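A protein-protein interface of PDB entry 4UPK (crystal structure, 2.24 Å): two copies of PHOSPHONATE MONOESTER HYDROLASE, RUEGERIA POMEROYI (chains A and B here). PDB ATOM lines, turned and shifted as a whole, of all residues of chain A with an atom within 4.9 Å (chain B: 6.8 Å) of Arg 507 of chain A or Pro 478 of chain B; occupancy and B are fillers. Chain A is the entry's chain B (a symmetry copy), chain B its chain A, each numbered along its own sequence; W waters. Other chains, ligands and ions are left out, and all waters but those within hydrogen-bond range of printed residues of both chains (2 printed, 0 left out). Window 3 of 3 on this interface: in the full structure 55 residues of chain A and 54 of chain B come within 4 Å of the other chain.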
ATOM      1  N   ALA A 503       7.551   7.080 -12.629  1.00  0.00           N
ATOM      2  CA  ALA A 503       7.208   6.240 -11.466  1.00  0.00           C
ATOM      3  C   ALA A 503       6.132   6.879 -10.597  1.00  0.00           C
ATOM      4  O   ALA A 503       5.205   6.180 -10.178  1.00  0.00           O
ATOM      5  CB  ALA A 503       8.456   5.936 -10.637  1.00  0.00           C
ATOM      6  N   ARG A 504       6.250   8.214 -10.340  1.00  0.00           N
ATOM      7  CA  ARG A 504       5.321   9.012  -9.534  1.00  0.00           C
ATOM      8  C   ARG A 504       3.929   9.091 -10.182  1.00  0.00           C
ATOM      9  O   ARG A 504       2.933   8.888  -9.488  1.00  0.00           O
ATOM     10  CB  ARG A 504       5.901  10.413  -9.297  1.00  0.00           C
ATOM     11  CG  ARG A 504       4.989  11.392  -8.531  1.00  0.00           C
ATOM     12  CD  ARG A 504       5.597  12.776  -8.384  1.00  0.00           C
ATOM     13  NE  ARG A 504       6.125  13.304  -9.649  1.00  0.00           N
ATOM     14  CZ  ARG A 504       5.423  14.026 -10.510  1.00  0.00           C
ATOM     15  NH1 ARG A 504       4.153  14.324 -10.259  1.00  0.00           N
ATOM     16  NH2 ARG A 504       5.982  14.451 -11.639  1.00  0.00           N
ATOM     17  N   LEU A 505       3.866   9.371 -11.509  1.00  0.00           N
ATOM     18  CA  LEU A 505       2.608   9.465 -12.249  1.00  0.00           C
ATOM     19  C   LEU A 505       1.886   8.129 -12.380  1.00  0.00           C
ATOM     20  O   LEU A 505       0.661   8.090 -12.289  1.00  0.00           O
ATOM     21  CB  LEU A 505       2.807  10.120 -13.625  1.00  0.00           C
ATOM     22  CG  LEU A 505       3.132  11.610 -13.620  1.00  0.00           C
ATOM     23  CD1 LEU A 505       3.877  11.976 -14.846  1.00  0.00           C
ATOM     24  CD2 LEU A 505       1.902  12.446 -13.454  1.00  0.00           C
ATOM     25  N   SER A 506       2.647   7.040 -12.608  1.00  0.00           N
ATOM     26  CA  SER A 506       2.134   5.673 -12.716  1.00  0.00           C
ATOM     27  C   SER A 506       1.549   5.191 -11.370  1.00  0.00           C
ATOM     28  O   SER A 506       0.512   4.517 -11.365  1.00  0.00           O
ATOM     29  CB  SER A 506       3.216   4.738 -13.240  1.00  0.00           C
ATOM     30  OG  SER A 506       2.635   3.636 -13.920  1.00  0.00           O
ATOM     31  N   ARG A 507       2.142   5.606 -10.241  1.00  0.00           N
ATOM     32  CA  ARG A 507       1.609   5.271  -8.915  1.00  0.00           C
ATOM     33  C   ARG A 507       0.322   6.049  -8.682  1.00  0.00           C
ATOM     34  O   ARG A 507      -0.655   5.487  -8.169  1.00  0.00           O
ATOM     35  CB  ARG A 507       2.637   5.501  -7.794  1.00  0.00           C
ATOM     36  CG  ARG A 507       2.153   5.095  -6.388  1.00  0.00           C
ATOM     37  CD  ARG A 507       3.184   4.308  -5.570  1.00  0.00           C
ATOM     38  NE  ARG A 507       4.535   4.772  -5.859  1.00  0.00           N
ATOM     39  CZ  ARG A 507       5.538   4.007  -6.242  1.00  0.00           C
ATOM     40  NH1 ARG A 507       5.382   2.696  -6.347  1.00  0.00           N
ATOM     41  NH2 ARG A 507       6.715   4.544  -6.514  1.00  0.00           N
ATOM     42  N   GLN A 508       0.300   7.310  -9.137  1.00  0.00           N
ATOM     43  CA  GLN A 508      -0.872   8.185  -9.097  1.00  0.00           C
ATOM     44  C   GLN A 508      -2.012   7.571  -9.940  1.00  0.00           C
ATOM     45  O   GLN A 508      -3.165   7.576  -9.500  1.00  0.00           O
ATOM     46  CB  GLN A 508      -0.482   9.590  -9.587  1.00  0.00           C
ATOM     47  CG  GLN A 508      -1.549  10.645  -9.377  1.00  0.00           C
ATOM     48  CD  GLN A 508      -0.976  12.039  -9.320  1.00  0.00           C
ATOM     49  OE1 GLN A 508       0.023  12.374  -9.977  1.00  0.00           O
ATOM     50  NE2 GLN A 508      -1.630  12.896  -8.548  1.00  0.00           N
ATOM     51  N   MET A 509      -1.674   6.986 -11.114  1.00  0.00           N
ATOM     52  CA  MET A 509      -2.607   6.273 -11.991  1.00  0.00           C
ATOM     53  C   MET A 509      -3.098   4.968 -11.341  1.00  0.00           C
ATOM     54  O   MET A 509      -4.287   4.662 -11.430  1.00  0.00           O
ATOM     55  CB  MET A 509      -1.972   5.978 -13.357  1.00  0.00           C
ATOM     56  CG  MET A 509      -2.945   5.295 -14.319  1.00  0.00           C
ATOM     57  SD  MET A 509      -2.249   4.862 -15.910  1.00  0.00           S
ATOM     58  CE  MET A 509      -2.459   6.420 -16.791  1.00  0.00           C
ATOM     59  N   LEU A 510      -2.179   4.200 -10.708  1.00  0.00           N
ATOM     60  CA  LEU A 510      -2.496   2.965 -10.004  1.00  0.00           C
ATOM     61  C   LEU A 510      -3.489   3.277  -8.872  1.00  0.00           C
ATOM     62  O   LEU A 510      -4.528   2.618  -8.767  1.00  0.00           O
ATOM     63  CB  LEU A 510      -1.212   2.295  -9.443  1.00  0.00           C
ATOM     64  CG  LEU A 510      -1.418   0.995  -8.605  1.00  0.00           C
ATOM     65  CD1 LEU A 510      -1.882  -0.162  -9.473  1.00  0.00           C
ATOM     66  CD2 LEU A 510      -0.154   0.586  -7.903  1.00  0.00           C
ATOM     67  N   ARG A 511      -3.185   4.303  -8.056  1.00  0.00           N
ATOM     68  CA  ARG A 511      -4.051   4.748  -6.955  1.00  0.00           C
ATOM     69  C   ARG A 511      -5.442   5.161  -7.418  1.00  0.00           C
ATOM     70  O   ARG A 511      -6.408   4.840  -6.729  1.00  0.00           O
ATOM     71  CB  ARG A 511      -3.403   5.881  -6.159  1.00  0.00           C
ATOM     72  CG  ARG A 511      -2.251   5.407  -5.285  1.00  0.00           C
ATOM     73  CD  ARG A 511      -1.937   6.414  -4.198  1.00  0.00           C
ATOM     74  NE  ARG A 511      -0.983   5.861  -3.233  1.00  0.00           N
ATOM     75  CZ  ARG A 511       0.218   6.370  -2.985  1.00  0.00           C
ATOM     76  NH1 ARG A 511       0.618   7.471  -3.599  1.00  0.00           N
ATOM     77  NH2 ARG A 511       1.018   5.799  -2.096  1.00  0.00           N
ATOM     78  N   GLU B 276       9.365  -0.845  10.008  1.00  0.00           N
ATOM     79  CA  GLU B 276       9.418  -1.347   8.639  1.00  0.00           C
ATOM     80  C   GLU B 276       8.402  -0.650   7.718  1.00  0.00           C
ATOM     81  O   GLU B 276       8.725  -0.342   6.569  1.00  0.00           O
ATOM     82  CB  GLU B 276       9.351  -2.886   8.572  1.00  0.00           C
ATOM     83  CG  GLU B 276      10.593  -3.587   9.122  1.00  0.00           C
ATOM     84  CD  GLU B 276      11.936  -3.119   8.595  1.00  0.00           C
ATOM     85  OE1 GLU B 276      12.094  -3.005   7.360  1.00  0.00           O
ATOM     86  OE2 GLU B 276      12.844  -2.888   9.422  1.00  0.00           O
ATOM     87  N   HIS B 277       7.203  -0.322   8.252  1.00  0.00           N
ATOM     88  CA  HIS B 277       6.167   0.441   7.548  1.00  0.00           C
ATOM     89  C   HIS B 277       5.093   0.829   8.581  1.00  0.00           C
ATOM     90  O   HIS B 277       4.736  -0.006   9.418  1.00  0.00           O
ATOM     91  CB  HIS B 277       5.570  -0.336   6.339  1.00  0.00           C
ATOM     92  CG  HIS B 277       4.715   0.479   5.404  1.00  0.00           C
ATOM     93  ND1 HIS B 277       3.426   0.883   5.759  1.00  0.00           N
ATOM     94  CD2 HIS B 277       4.959   0.884   4.133  1.00  0.00           C
ATOM     95  CE1 HIS B 277       2.958   1.555   4.718  1.00  0.00           C
ATOM     96  NE2 HIS B 277       3.839   1.570   3.710  1.00  0.00           N
ATOM     97  N   LEU B 469       5.666  -6.994  -3.604  1.00  0.00           N
ATOM     98  CA  LEU B 469       5.324  -5.585  -3.638  1.00  0.00           C
ATOM     99  C   LEU B 469       3.950  -5.385  -2.967  1.00  0.00           C
ATOM    100  O   LEU B 469       3.018  -6.151  -3.224  1.00  0.00           O
ATOM    101  CB  LEU B 469       5.296  -5.081  -5.107  1.00  0.00           C
ATOM    102  CG  LEU B 469       4.669  -3.692  -5.349  1.00  0.00           C
ATOM    103  CD1 LEU B 469       5.629  -2.560  -5.001  1.00  0.00           C
ATOM    104  CD2 LEU B 469       4.214  -3.570  -6.732  1.00  0.00           C
ATOM    105  N   VAL B 470       3.845  -4.348  -2.110  1.00  0.00           N
ATOM    106  CA  VAL B 470       2.608  -3.939  -1.456  1.00  0.00           C
ATOM    107  C   VAL B 470       2.337  -2.490  -1.892  1.00  0.00           C
ATOM    108  O   VAL B 470       3.203  -1.633  -1.748  1.00  0.00           O
ATOM    109  CB  VAL B 470       2.625  -4.097   0.088  1.00  0.00           C
ATOM    110  CG1 VAL B 470       1.330  -3.576   0.717  1.00  0.00           C
ATOM    111  CG2 VAL B 470       2.887  -5.554   0.511  1.00  0.00           C
ATOM    112  N   GLU B 471       1.137  -2.223  -2.450  1.00  0.00           N
ATOM    113  CA  GLU B 471       0.737  -0.872  -2.859  1.00  0.00           C
ATOM    114  C   GLU B 471      -0.591  -0.509  -2.229  1.00  0.00           C
ATOM    115  O   GLU B 471      -1.515  -1.328  -2.223  1.00  0.00           O
ATOM    116  CB  GLU B 471       0.652  -0.755  -4.387  1.00  0.00           C
ATOM    117  CG  GLU B 471       2.003  -0.851  -5.085  1.00  0.00           C
ATOM    118  CD  GLU B 471       2.799   0.432  -5.218  1.00  0.00           C
ATOM    119  OE1 GLU B 471       2.441   1.442  -4.566  1.00  0.00           O
ATOM    120  OE2 GLU B 471       3.781   0.423  -5.995  1.00  0.00           O
ATOM    121  N   PHE B 472      -0.690   0.720  -1.715  1.00  0.00           N
ATOM    122  CA  PHE B 472      -1.894   1.272  -1.067  1.00  0.00           C
ATOM    123  C   PHE B 472      -2.632   2.274  -1.972  1.00  0.00           C
ATOM    124  O   PHE B 472      -1.989   3.058  -2.659  1.00  0.00           O
ATOM    125  CB  PHE B 472      -1.488   2.014   0.232  1.00  0.00           C
ATOM    126  CG  PHE B 472      -0.893   1.115   1.283  1.00  0.00           C
ATOM    127  CD1 PHE B 472       0.476   0.858   1.310  1.00  0.00           C
ATOM    128  CD2 PHE B 472      -1.703   0.491   2.222  1.00  0.00           C
ATOM    129  CE1 PHE B 472       1.017  -0.001   2.256  1.00  0.00           C
ATOM    130  CE2 PHE B 472      -1.153  -0.356   3.184  1.00  0.00           C
ATOM    131  CZ  PHE B 472       0.201  -0.587   3.200  1.00  0.00           C
ATOM    132  N   LEU B 476      -0.023   6.113   1.471  1.00  0.00           N
ATOM    133  CA  LEU B 476       0.960   5.355   2.255  1.00  0.00           C
ATOM    134  C   LEU B 476       1.980   4.782   1.284  1.00  0.00           C
ATOM    135  O   LEU B 476       1.580   4.289   0.225  1.00  0.00           O
ATOM    136  CB  LEU B 476       0.291   4.217   3.032  1.00  0.00           C
ATOM    137  CG  LEU B 476      -0.537   4.599   4.249  1.00  0.00           C
ATOM    138  CD1 LEU B 476      -1.262   3.382   4.788  1.00  0.00           C
ATOM    139  CD2 LEU B 476       0.335   5.229   5.359  1.00  0.00           C
ATOM    140  N   PRO B 477       3.294   4.841   1.589  1.00  0.00           N
ATOM    141  CA  PRO B 477       4.284   4.334   0.628  1.00  0.00           C
ATOM    142  C   PRO B 477       4.246   2.819   0.374  1.00  0.00           C
ATOM    143  O   PRO B 477       3.771   2.050   1.213  1.00  0.00           O
ATOM    144  CB  PRO B 477       5.632   4.784   1.228  1.00  0.00           C
ATOM    145  CG  PRO B 477       5.377   4.957   2.671  1.00  0.00           C
ATOM    146  CD  PRO B 477       3.957   5.438   2.776  1.00  0.00           C
ATOM    147  N   PRO B 478       4.773   2.358  -0.792  1.00  0.00           N
ATOM    148  CA  PRO B 478       4.802   0.912  -1.041  1.00  0.00           C
ATOM    149  C   PRO B 478       5.746   0.145  -0.108  1.00  0.00           C
ATOM    150  O   PRO B 478       6.570   0.744   0.597  1.00  0.00           O
ATOM    151  CB  PRO B 478       5.301   0.814  -2.489  1.00  0.00           C
ATOM    152  CG  PRO B 478       6.025   2.070  -2.746  1.00  0.00           C
ATOM    153  CD  PRO B 478       5.349   3.120  -1.924  1.00  0.00           C
ATOM    154  N   MET B 479       5.611  -1.184  -0.106  1.00  0.00           N
ATOM    155  CA  MET B 479       6.513  -2.074   0.595  1.00  0.00           C
ATOM    156  C   MET B 479       7.183  -2.919  -0.470  1.00  0.00           C
ATOM    157  O   MET B 479       6.573  -3.244  -1.482  1.00  0.00           O
ATOM    158  CB  MET B 479       5.799  -2.997   1.617  1.00  0.00           C
ATOM    159  CG  MET B 479       4.879  -2.283   2.562  1.00  0.00           C
ATOM    160  SD  MET B 479       4.402  -3.346   3.915  1.00  0.00           S
ATOM    161  CE  MET B 479       2.940  -2.541   4.498  1.00  0.00           C
ATOM    162  N   LEU B 480       8.430  -3.255  -0.258  1.00  0.00           N
ATOM    163  CA  LEU B 480       9.159  -4.121  -1.170  1.00  0.00           C
ATOM    164  C   LEU B 480      10.021  -5.094  -0.374  1.00  0.00           C
ATOM    165  O   LEU B 480      10.857  -4.663   0.398  1.00  0.00           O
ATOM    166  CB  LEU B 480       9.964  -3.334  -2.193  1.00  0.00           C
ATOM    167  CG  LEU B 480      10.604  -4.176  -3.310  1.00  0.00           C
ATOM    168  CD1 LEU B 480       9.557  -4.734  -4.245  1.00  0.00           C
ATOM    169  CD2 LEU B 480      11.654  -3.363  -4.055  1.00  0.00           C
ATOM    170  N   ASN B 491      11.598  -4.076   4.747  1.00  0.00           N
ATOM    171  CA  ASN B 491      10.950  -3.331   3.673  1.00  0.00           C
ATOM    172  C   ASN B 491      12.068  -2.495   3.003  1.00  0.00           C
ATOM    173  O   ASN B 491      12.621  -1.579   3.627  1.00  0.00           O
ATOM    174  CB  ASN B 491       9.786  -2.455   4.197  1.00  0.00           C
ATOM    175  CG  ASN B 491       9.271  -1.427   3.224  1.00  0.00           C
ATOM    176  OD1 ASN B 491       9.438  -1.554   2.009  1.00  0.00           O
ATOM    177  ND2 ASN B 491       8.619  -0.388   3.734  1.00  0.00           N
ATOM    178  N   VAL B 492      12.405  -2.835   1.742  1.00  0.00           N
ATOM    179  CA  VAL B 492      13.467  -2.180   0.979  1.00  0.00           C
ATOM    180  C   VAL B 492      12.976  -1.162  -0.072  1.00  0.00           C
ATOM    181  O   VAL B 492      13.775  -0.731  -0.902  1.00  0.00           O
ATOM    182  CB  VAL B 492      14.508  -3.194   0.412  1.00  0.00           C
ATOM    183  CG1 VAL B 492      15.229  -3.937   1.533  1.00  0.00           C
ATOM    184  CG2 VAL B 492      13.879  -4.181  -0.567  1.00  0.00           C
ATOM    185  N   ALA B 493      11.682  -0.757  -0.026  1.00  0.00           N
ATOM    186  CA  ALA B 493      11.095   0.190  -0.987  1.00  0.00           C
ATOM    187  C   ALA B 493      11.748   1.586  -1.026  1.00  0.00           C
ATOM    188  O   ALA B 493      11.704   2.248  -2.063  1.00  0.00           O
ATOM    189  CB  ALA B 493       9.584   0.296  -0.788  1.00  0.00           C
ATOM    190  N   GLY B 494      12.329   2.030   0.086  1.00  0.00           N
ATOM    191  CA  GLY B 494      12.998   3.332   0.157  1.00  0.00           C
ATOM    192  C   GLY B 494      14.455   3.319  -0.290  1.00  0.00           C
ATOM    193  O   GLY B 494      15.077   4.376  -0.411  1.00  0.00           O
ATOM    194  N   LEU B 502      11.133  -1.662  -8.048  1.00  0.00           N
ATOM    195  CA  LEU B 502       9.887  -1.071  -7.531  1.00  0.00           C
ATOM    196  C   LEU B 502       8.999  -0.578  -8.686  1.00  0.00           C
ATOM    197  O   LEU B 502       7.811  -0.917  -8.729  1.00  0.00           O
ATOM    198  CB  LEU B 502      10.222   0.087  -6.547  1.00  0.00           C
ATOM    199  CG  LEU B 502       9.063   0.803  -5.827  1.00  0.00           C
ATOM    200  CD1 LEU B 502       8.383  -0.116  -4.829  1.00  0.00           C
ATOM    201  CD2 LEU B 502       9.562   2.044  -5.118  1.00  0.00           C
ATOM    202  N   ALA B 503       9.586   0.191  -9.634  1.00  0.00           N
ATOM    203  CA  ALA B 503       8.872   0.717 -10.795  1.00  0.00           C
ATOM    204  C   ALA B 503       8.362  -0.399 -11.736  1.00  0.00           C
ATOM    205  O   ALA B 503       7.229  -0.320 -12.238  1.00  0.00           O
ATOM    206  CB  ALA B 503       9.758   1.708 -11.544  1.00  0.00           C
ATOM    207  N   SER B 506       5.491  -2.491  -9.897  1.00  0.00           N
ATOM    208  CA  SER B 506       4.300  -1.642  -9.815  1.00  0.00           C
ATOM    209  C   SER B 506       3.594  -1.536 -11.192  1.00  0.00           C
ATOM    210  O   SER B 506       2.358  -1.523 -11.242  1.00  0.00           O
ATOM    211  CB  SER B 506       4.666  -0.273  -9.249  1.00  0.00           C
ATOM    212  OG  SER B 506       3.559   0.297  -8.575  1.00  0.00           O
ATOM    213  N   LEU B 510      -0.050  -2.720 -11.998  1.00  0.00           N
ATOM    214  CA  LEU B 510      -0.960  -1.852 -12.739  1.00  0.00           C
ATOM    215  C   LEU B 510      -1.589  -2.651 -13.887  1.00  0.00           C
ATOM    216  O   LEU B 510      -2.813  -2.680 -14.016  1.00  0.00           O
ATOM    217  CB  LEU B 510      -0.229  -0.583 -13.275  1.00  0.00           C
ATOM    218  CG  LEU B 510      -1.060   0.369 -14.165  1.00  0.00           C
ATOM    219  CD1 LEU B 510      -2.121   1.122 -13.349  1.00  0.00           C
ATOM    220  CD2 LEU B 510      -0.196   1.376 -14.844  1.00  0.00           C
HETATM  221  O   HOH W   1       3.186   2.566  -9.661  1.00  0.00           O
HETATM  222  O   HOH W   2       1.543   2.400  -2.135  1.00  0.00           O
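Ser 506 of chain A touches Leu 510 of chain B.
CG of Pro 478 of chain B touches NH1 of Arg 507 of chain A, 3.7 Å away.
Arg 507 of chain A touches Ser 506 of chain B.
Leu 510 of chain A touches Glu 471 of chain B.
Ser 506 of chain B touches Leu 510 of chain A.
Leu 510 of chain A touches Leu 510 of chain B.
OE2 of Glu 471 of chain B lies within salt-bridge range of NH1 of Arg 507 of chain A, 2.8 Å away.
O of Phe 472 of chain B sits at hydrogen-bond distance from NE of Arg 511 of chain A (3.0 Å).
The backbone carbonyl oxygen (O) of Leu 476 of chain B sits at hydrogen-bond distance from the guanidinium group (NH2) of Arg 511 of chain A, 2.8 Å away.
Water W1 bridges OG of Ser 506 of chain B (2.5 Å) and N of Arg 507 of chain A (3.3 Å).
Water W2 lies within hydrogen-bond range of OE1 of Glu 471 of chain B, N of Phe 472 of chain B, O of Leu 476 of chain B and NH2 of Arg 511 of chain A.
The side-chain carboxylate of Glu 471 of chain B is in hydrogen-bond range of the side-chain hydroxyl of Ser 506 of chain B (2.6 Å).
Of chain B, only Glu 471 (2.8 Å), Pro 478 (3.7 Å) and Ser 506 (3.7 Å) come within 4 Å of Arg 507 of chain A.
Pro 478 of chain B touches one residue of chain A.
Of the printed residues of chain B, Leu 510 of chain A touches Glu 471 (3.8 Å), Ser 506 (3.8 Å) and Leu 510 (3.8 Å).
Of the printed residues of chain A, Ser 506 of chain B touches Arg 507 and Leu 510.
Leu 502 of chain B touches none of the printed residues of chain A.
Of the 9 printed residues of chain A, 4 touch a printed residue of chain B.
Printed residues of chain A that touch a printed residue of chain B: Ser 506, Arg 507, Leu 510 and Arg 511.
Hydrophobic or aromatic side chains of chain A that line the printed part of chain B: Leu 510.
Ser 506 of chain A touches Leu 510 of chain B, and with the chains exchanged Leu 510 of chain A touches Ser 506 of chain B.
Leu 510 of chain A touches its own counterpart, Leu 510 of chain B.
Positions printed for both chains: 503, 506 and 510.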
